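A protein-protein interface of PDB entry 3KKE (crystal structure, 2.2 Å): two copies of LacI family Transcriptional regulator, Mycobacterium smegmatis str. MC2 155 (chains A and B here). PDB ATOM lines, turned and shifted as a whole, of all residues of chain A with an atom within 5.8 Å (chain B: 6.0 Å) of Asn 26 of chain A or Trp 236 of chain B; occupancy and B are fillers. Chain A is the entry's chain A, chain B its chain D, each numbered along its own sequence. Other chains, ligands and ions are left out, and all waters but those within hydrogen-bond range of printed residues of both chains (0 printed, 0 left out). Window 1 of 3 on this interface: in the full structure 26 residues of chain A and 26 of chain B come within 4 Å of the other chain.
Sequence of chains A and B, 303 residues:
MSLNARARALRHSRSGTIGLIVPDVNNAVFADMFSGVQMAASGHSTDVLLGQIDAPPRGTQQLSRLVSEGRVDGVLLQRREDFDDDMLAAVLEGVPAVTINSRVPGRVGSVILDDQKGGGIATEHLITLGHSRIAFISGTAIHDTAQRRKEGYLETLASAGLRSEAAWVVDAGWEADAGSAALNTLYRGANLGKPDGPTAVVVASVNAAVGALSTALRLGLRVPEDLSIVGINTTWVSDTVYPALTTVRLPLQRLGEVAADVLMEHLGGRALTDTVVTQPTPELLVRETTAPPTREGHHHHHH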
ATOM      1  N   ASP A  24      18.860   1.176 -12.301  1.00  0.00           N
ATOM      2  CA  ASP A  24      19.982   1.122 -11.350  1.00  0.00           C
ATOM      3  C   ASP A  24      20.009  -0.290 -10.776  1.00  0.00           C
ATOM      4  O   ASP A  24      18.971  -0.925 -10.587  1.00  0.00           O
ATOM      5  CB  ASP A  24      19.823   2.151 -10.213  1.00  0.00           C
ATOM      6  CG  ASP A  24      21.074   2.248  -9.280  1.00  0.00           C
ATOM      7  OD1 ASP A  24      21.460   1.236  -8.639  1.00  0.00           O
ATOM      8  OD2 ASP A  24      21.670   3.357  -9.143  1.00  0.00           O
ATOM      9  N   VAL A  25      21.199  -0.784 -10.477  1.00  0.00           N
ATOM     10  CA  VAL A  25      21.343  -2.124  -9.935  1.00  0.00           C
ATOM     11  C   VAL A  25      20.959  -2.188  -8.434  1.00  0.00           C
ATOM     12  O   VAL A  25      20.824  -3.270  -7.871  1.00  0.00           O
ATOM     13  CB  VAL A  25      22.760  -2.651 -10.177  1.00  0.00           C
ATOM     14  CG1 VAL A  25      23.111  -2.536 -11.673  1.00  0.00           C
ATOM     15  CG2 VAL A  25      23.777  -1.893  -9.307  1.00  0.00           C
ATOM     16  N   ASN A  26      20.758  -1.037  -7.804  1.00  0.00           N
ATOM     17  CA  ASN A  26      20.173  -0.972  -6.457  1.00  0.00           C
ATOM     18  C   ASN A  26      18.692  -1.254  -6.379  1.00  0.00           C
ATOM     19  O   ASN A  26      18.174  -1.420  -5.272  1.00  0.00           O
ATOM     20  CB  ASN A  26      20.364   0.427  -5.814  1.00  0.00           C
ATOM     21  CG  ASN A  26      21.474   0.450  -4.788  1.00  0.00           C
ATOM     22  OD1 ASN A  26      21.773  -0.558  -4.139  1.00  0.00           O
ATOM     23  ND2 ASN A  26      22.078   1.601  -4.631  1.00  0.00           N
ATOM     24  N   ASN A  27      18.011  -1.258  -7.522  1.00  0.00           N
ATOM     25  CA  ASN A  27      16.572  -1.497  -7.570  1.00  0.00           C
ATOM     26  C   ASN A  27      16.200  -2.834  -6.879  1.00  0.00           C
ATOM     27  O   ASN A  27      16.925  -3.823  -6.987  1.00  0.00           O
ATOM     28  CB  ASN A  27      16.079  -1.328  -9.038  1.00  0.00           C
ATOM     29  CG  ASN A  27      14.890  -2.211  -9.403  1.00  0.00           C
ATOM     30  OD1 ASN A  27      15.071  -3.385  -9.727  1.00  0.00           O
ATOM     31  ND2 ASN A  27      13.665  -1.634  -9.412  1.00  0.00           N
ATOM     32  N   ALA A  28      15.078  -2.816  -6.142  1.00  0.00           N
ATOM     33  CA  ALA A  28      14.604  -3.941  -5.312  1.00  0.00           C
ATOM     34  C   ALA A  28      14.456  -5.276  -6.041  1.00  0.00           C
ATOM     35  O   ALA A  28      14.751  -6.344  -5.491  1.00  0.00           O
ATOM     36  CB  ALA A  28      13.257  -3.587  -4.719  1.00  0.00           C
ATOM     37  N   PHE A  30      15.990  -6.094  -8.806  1.00  0.00           N
ATOM     38  CA  PHE A  30      17.155  -6.434  -9.642  1.00  0.00           C
ATOM     39  C   PHE A  30      17.773  -7.792  -9.357  1.00  0.00           C
ATOM     40  O   PHE A  30      17.935  -8.593 -10.256  1.00  0.00           O
ATOM     41  CB  PHE A  30      18.251  -5.377  -9.547  1.00  0.00           C
ATOM     42  CG  PHE A  30      19.461  -5.705 -10.373  1.00  0.00           C
ATOM     43  CD1 PHE A  30      19.425  -5.559 -11.759  1.00  0.00           C
ATOM     44  CD2 PHE A  30      20.615  -6.192  -9.771  1.00  0.00           C
ATOM     45  CE1 PHE A  30      20.550  -5.865 -12.546  1.00  0.00           C
ATOM     46  CE2 PHE A  30      21.752  -6.506 -10.530  1.00  0.00           C
ATOM     47  CZ  PHE A  30      21.721  -6.335 -11.929  1.00  0.00           C
ATOM     48  N   GLN A  52      23.214   0.293 -17.426  1.00  0.00           N
ATOM     49  CA  GLN A  52      22.535   1.097 -16.443  1.00  0.00           C
ATOM     50  C   GLN A  52      22.360   2.471 -17.030  1.00  0.00           C
ATOM     51  O   GLN A  52      23.365   3.079 -17.449  1.00  0.00           O
ATOM     52  CB  GLN A  52      23.412   1.206 -15.205  1.00  0.00           C
ATOM     53  CG  GLN A  52      22.771   1.883 -14.045  1.00  0.00           C
ATOM     54  CD  GLN A  52      23.592   1.731 -12.791  1.00  0.00           C
ATOM     55  OE1 GLN A  52      23.272   0.917 -11.921  1.00  0.00           O
ATOM     56  NE2 GLN A  52      24.674   2.498 -12.694  1.00  0.00           N
ATOM     57  N   GLU A 175      11.460   3.960  -4.720  1.00  0.00           N
ATOM     58  CA  GLU A 175      12.602   3.993  -3.801  1.00  0.00           C
ATOM     59  C   GLU A 175      12.273   4.603  -2.458  1.00  0.00           C
ATOM     60  O   GLU A 175      11.262   5.278  -2.298  1.00  0.00           O
ATOM     61  CB  GLU A 175      13.787   4.717  -4.437  1.00  0.00           C
ATOM     62  CG  GLU A 175      14.243   4.106  -5.781  1.00  0.00           C
ATOM     63  CD  GLU A 175      14.552   2.599  -5.710  1.00  0.00           C
ATOM     64  OE1 GLU A 175      15.120   2.137  -4.701  1.00  0.00           O
ATOM     65  OE2 GLU A 175      14.222   1.872  -6.672  1.00  0.00           O
ATOM     66  N   ALA A 176      13.163   4.350  -1.507  1.00  0.00           N
ATOM     67  CA  ALA A 176      13.006   4.779  -0.136  1.00  0.00           C
ATOM     68  C   ALA A 176      12.648   6.253   0.012  1.00  0.00           C
ATOM     69  O   ALA A 176      11.669   6.583   0.689  1.00  0.00           O
ATOM     70  CB  ALA A 176      14.258   4.453   0.673  1.00  0.00           C
ATOM     71  N   ASN A 207      11.069  -0.943  -1.449  1.00  0.00           N
ATOM     72  CA  ASN A 207      12.045   0.021  -0.963  1.00  0.00           C
ATOM     73  C   ASN A 207      11.357   1.265  -0.489  1.00  0.00           C
ATOM     74  O   ASN A 207      11.713   1.793   0.569  1.00  0.00           O
ATOM     75  CB  ASN A 207      13.126   0.398  -2.000  1.00  0.00           C
ATOM     76  CG  ASN A 207      14.126  -0.731  -2.259  1.00  0.00           C
ATOM     77  OD1 ASN A 207      14.069  -1.773  -1.633  1.00  0.00           O
ATOM     78  ND2 ASN A 207      14.997  -0.538  -3.238  1.00  0.00           N
ATOM     79  N   VAL A 210      10.100   0.613   2.876  1.00  0.00           N
ATOM     80  CA  VAL A 210      11.114   0.724   3.926  1.00  0.00           C
ATOM     81  C   VAL A 210      11.319   2.176   4.316  1.00  0.00           C
ATOM     82  O   VAL A 210      11.382   2.500   5.502  1.00  0.00           O
ATOM     83  CB  VAL A 210      12.448   0.095   3.475  1.00  0.00           C
ATOM     84  CG1 VAL A 210      13.561   0.347   4.544  1.00  0.00           C
ATOM     85  CG2 VAL A 210      12.249  -1.396   3.221  1.00  0.00           C
ATOM     86  N   GLY A 211      11.387   3.046   3.311  1.00  0.00           N
ATOM     87  CA  GLY A 211      11.317   4.490   3.532  1.00  0.00           C
ATOM     88  C   GLY A 211      10.072   4.939   4.300  1.00  0.00           C
ATOM     89  O   GLY A 211      10.153   5.742   5.232  1.00  0.00           O
ATOM     90  N   VAL A 237      16.206  -6.772   3.141  1.00  0.00           N
ATOM     91  CA  VAL A 237      15.960  -5.558   3.911  1.00  0.00           C
ATOM     92  C   VAL A 237      14.583  -5.568   4.562  1.00  0.00           C
ATOM     93  O   VAL A 237      14.442  -5.221   5.736  1.00  0.00           O
ATOM     94  CB  VAL A 237      16.046  -4.316   3.011  1.00  0.00           C
ATOM     95  CG1 VAL A 237      15.798  -3.039   3.812  1.00  0.00           C
ATOM     96  CG2 VAL A 237      17.412  -4.282   2.228  1.00  0.00           C
ATOM     97  N   ALA B  31      26.606  -1.962  -5.930  1.00  0.00           N
ATOM     98  CA  ALA B  31      26.000  -0.882  -6.700  1.00  0.00           C
ATOM     99  C   ALA B  31      27.026   0.183  -7.077  1.00  0.00           C
ATOM    100  O   ALA B  31      27.164   0.521  -8.247  1.00  0.00           O
ATOM    101  CB  ALA B  31      24.812  -0.235  -5.952  1.00  0.00           C
ATOM    102  N   ASP B  32      27.729   0.721  -6.082  1.00  0.00           N
ATOM    103  CA  ASP B  32      28.654   1.839  -6.313  1.00  0.00           C
ATOM    104  C   ASP B  32      29.853   1.431  -7.145  1.00  0.00           C
ATOM    105  O   ASP B  32      30.230   2.125  -8.084  1.00  0.00           O
ATOM    106  CB  ASP B  32      29.091   2.467  -4.987  1.00  0.00           C
ATOM    107  CG  ASP B  32      28.021   3.379  -4.403  1.00  0.00           C
ATOM    108  OD1 ASP B  32      27.111   3.781  -5.166  1.00  0.00           O
ATOM    109  OD2 ASP B  32      28.089   3.720  -3.198  1.00  0.00           O
ATOM    110  N   THR B 234      28.548   2.417   3.408  1.00  0.00           N
ATOM    111  CA  THR B 234      27.287   3.118   3.524  1.00  0.00           C
ATOM    112  C   THR B 234      26.349   2.807   2.336  1.00  0.00           C
ATOM    113  O   THR B 234      26.753   2.927   1.179  1.00  0.00           O
ATOM    114  CB  THR B 234      27.537   4.650   3.516  1.00  0.00           C
ATOM    115  OG1 THR B 234      28.430   5.003   4.582  1.00  0.00           O
ATOM    116  CG2 THR B 234      26.254   5.404   3.666  1.00  0.00           C
ATOM    117  N   THR B 235      25.088   2.481   2.617  1.00  0.00           N
ATOM    118  CA  THR B 235      24.111   2.276   1.560  1.00  0.00           C
ATOM    119  C   THR B 235      22.871   3.093   1.842  1.00  0.00           C
ATOM    120  O   THR B 235      22.738   3.678   2.923  1.00  0.00           O
ATOM    121  CB  THR B 235      23.715   0.797   1.472  1.00  0.00           C
ATOM    122  OG1 THR B 235      23.181   0.385   2.742  1.00  0.00           O
ATOM    123  CG2 THR B 235      24.944  -0.043   1.129  1.00  0.00           C
ATOM    124  N   TRP B 236      21.932   3.076   0.910  1.00  0.00           N
ATOM    125  CA  TRP B 236      20.644   3.707   1.150  1.00  0.00           C
ATOM    126  C   TRP B 236      19.964   3.033   2.334  1.00  0.00           C
ATOM    127  O   TRP B 236      19.195   3.662   3.072  1.00  0.00           O
ATOM    128  CB  TRP B 236      19.766   3.693  -0.108  1.00  0.00           C
ATOM    129  CG  TRP B 236      19.274   2.359  -0.491  1.00  0.00           C
ATOM    130  CD1 TRP B 236      19.829   1.523  -1.403  1.00  0.00           C
ATOM    131  CD2 TRP B 236      18.118   1.696   0.023  1.00  0.00           C
ATOM    132  NE1 TRP B 236      19.104   0.357  -1.472  1.00  0.00           N
ATOM    133  CE2 TRP B 236      18.031   0.450  -0.627  1.00  0.00           C
ATOM    134  CE3 TRP B 236      17.154   2.029   0.978  1.00  0.00           C
ATOM    135  CZ2 TRP B 236      17.038  -0.472  -0.341  1.00  0.00           C
ATOM    136  CZ3 TRP B 236      16.147   1.119   1.252  1.00  0.00           C
ATOM    137  CH2 TRP B 236      16.101  -0.123   0.602  1.00  0.00           C
ATOM    138  N   VAL B 237      20.290   1.765   2.569  1.00  0.00           N
ATOM    139  CA  VAL B 237      19.686   1.055   3.710  1.00  0.00           C
ATOM    140  C   VAL B 237      20.139   1.580   5.073  1.00  0.00           C
ATOM    141  O   VAL B 237      19.319   1.767   5.976  1.00  0.00           O
ATOM    142  CB  VAL B 237      19.969  -0.452   3.673  1.00  0.00           C
ATOM    143  CG1 VAL B 237      19.321  -1.140   4.894  1.00  0.00           C
ATOM    144  CG2 VAL B 237      19.500  -1.042   2.371  1.00  0.00           C
ATOM    145  N   SER B 238      21.447   1.782   5.225  1.00  0.00           N
ATOM    146  CA  SER B 238      22.004   2.262   6.505  1.00  0.00           C
ATOM    147  C   SER B 238      21.559   3.686   6.810  1.00  0.00           C
ATOM    148  O   SER B 238      21.400   4.056   7.968  1.00  0.00           O
ATOM    149  CB  SER B 238      23.540   2.182   6.518  1.00  0.00           C
ATOM    150  OG  SER B 238      24.116   2.970   5.489  1.00  0.00           O
ATOM    151  N   ASP B 239      21.363   4.475   5.764  1.00  0.00           N
ATOM    152  CA  ASP B 239      20.816   5.814   5.904  1.00  0.00           C
ATOM    153  C   ASP B 239      19.320   5.879   6.102  1.00  0.00           C
ATOM    154  O   ASP B 239      18.820   6.893   6.605  1.00  0.00           O
ATOM    155  CB  ASP B 239      21.138   6.637   4.674  1.00  0.00           C
ATOM    156  CG  ASP B 239      22.512   7.243   4.726  1.00  0.00           C
ATOM    157  OD1 ASP B 239      23.113   7.349   5.841  1.00  0.00           O
ATOM    158  OD2 ASP B 239      22.987   7.625   3.636  1.00  0.00           O
ATOM    159  N   THR B 240      18.600   4.838   5.700  1.00  0.00           N
ATOM    160  CA  THR B 240      17.159   4.927   5.657  1.00  0.00           C
ATOM    161  C   THR B 240      16.513   4.399   6.929  1.00  0.00           C
ATOM    162  O   THR B 240      15.504   4.954   7.363  1.00  0.00           O
ATOM    163  CB  THR B 240      16.528   4.221   4.386  1.00  0.00           C
ATOM    164  OG1 THR B 240      17.035   4.822   3.185  1.00  0.00           O
ATOM    165  CG2 THR B 240      15.004   4.352   4.381  1.00  0.00           C
ATOM    166  N   VAL B 241      17.073   3.342   7.510  1.00  0.00           N
ATOM    167  CA  VAL B 241      16.481   2.700   8.686  1.00  0.00           C
ATOM    168  C   VAL B 241      16.409   3.639   9.932  1.00  0.00           C
ATOM    169  O   VAL B 241      17.034   4.681   9.963  1.00  0.00           O
ATOM    170  CB  VAL B 241      17.186   1.355   9.012  1.00  0.00           C
ATOM    171  CG1 VAL B 241      17.141   0.443   7.803  1.00  0.00           C
ATOM    172  CG2 VAL B 241      18.621   1.541   9.434  1.00  0.00           C
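Val 237 of chain A touches its own counterpart, Val 237 of chain B.
1 position is printed for both chains.
Of the 8 pairs that touch across the chains among the printed residues, 1 has its exchanged pair printed and touching as well.
Val 25 of chain A touches Ala 31 of chain B.
Asn 26 of chain A touches Ala 31 of chain B (ND2 to CB, 3.5 Å).
Asn 26 of chain A touches Trp 236 of chain B.
Trp 236 of chain B touches Ala 176 of chain A (CE3 to CB, 3.8 Å).
Ala 176 of chain A touches Thr 240 of chain B (CB to OG1, 3.8 Å).
OD1 of Asn 207 of chain A touches CH2 of Trp 236 of chain B (3.4 Å).
CG2 of Thr 240 of chain B touches CA of Gly 211 of chain A (3.8 Å).
CG2 of Val 237 of chain B touches CG2 of Val 237 of chain A, at 3.9 Å.
Asn 26 of chain A touches just these residues of chain B: Ala 31 and Trp 236.
Of the printed residues of chain B, Asn 207 of chain A touches Trp 236.
Trp 236 of chain B touches just these residues of chain A: Asn 26, Ala 176 and Asn 207.
Printed residues of chain A within 4 Å of Thr 240 of chain B: Ala 176 and Gly 211.
The side-chain amide oxygen of Gln 52 of chain A sits at hydrogen-bond distance from the backbone NH of Val 25 of chain A.
The side-chain carboxylate (OE1) of Glu 175 of chain A lies within hydrogen-bond range of the side-chain amide nitrogen (ND2) of Asn 207 of chain A (3.1 Å).
The backbone carbonyl oxygen (O) of Trp 236 of chain B sits at hydrogen-bond distance from the side-chain hydroxyl (OG1) of Thr 240 of chain B, at 2.5 Å.
The backbone NH (N) of Asn 26 of chain A sits at hydrogen-bond distance from the side-chain carboxylate (OD1) of Asp 24 of chain A (2.5 Å).
The side-chain hydroxyl (OG1) of Thr 235 of chain B lies close to the backbone NH (N) of Val 237 of chain B.
Printed residues of chain A that touch a printed residue of chain B: Val 25, Asn 26, Ala 176, Asn 207, Gly 211 and Val 237.
Hydrophobic or aromatic side chains of chain A that line the printed part of chain B: Val 25, Ala 176 and Val 237.
Of the 10 printed residues of chain B, 4 touch a printed residue of chain A.
Hydrophobic or aromatic side chains of chain B within 4 Å of the printed part of chain A: Ala 31, Trp 236 and Val 237.
Among the printed residues, 8 pairs touch across the chains.
Among the printed residues, no Asp or Glu carboxylate lies within 4 Å of a Lys or Arg side-chain nitrogen of the other chain.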
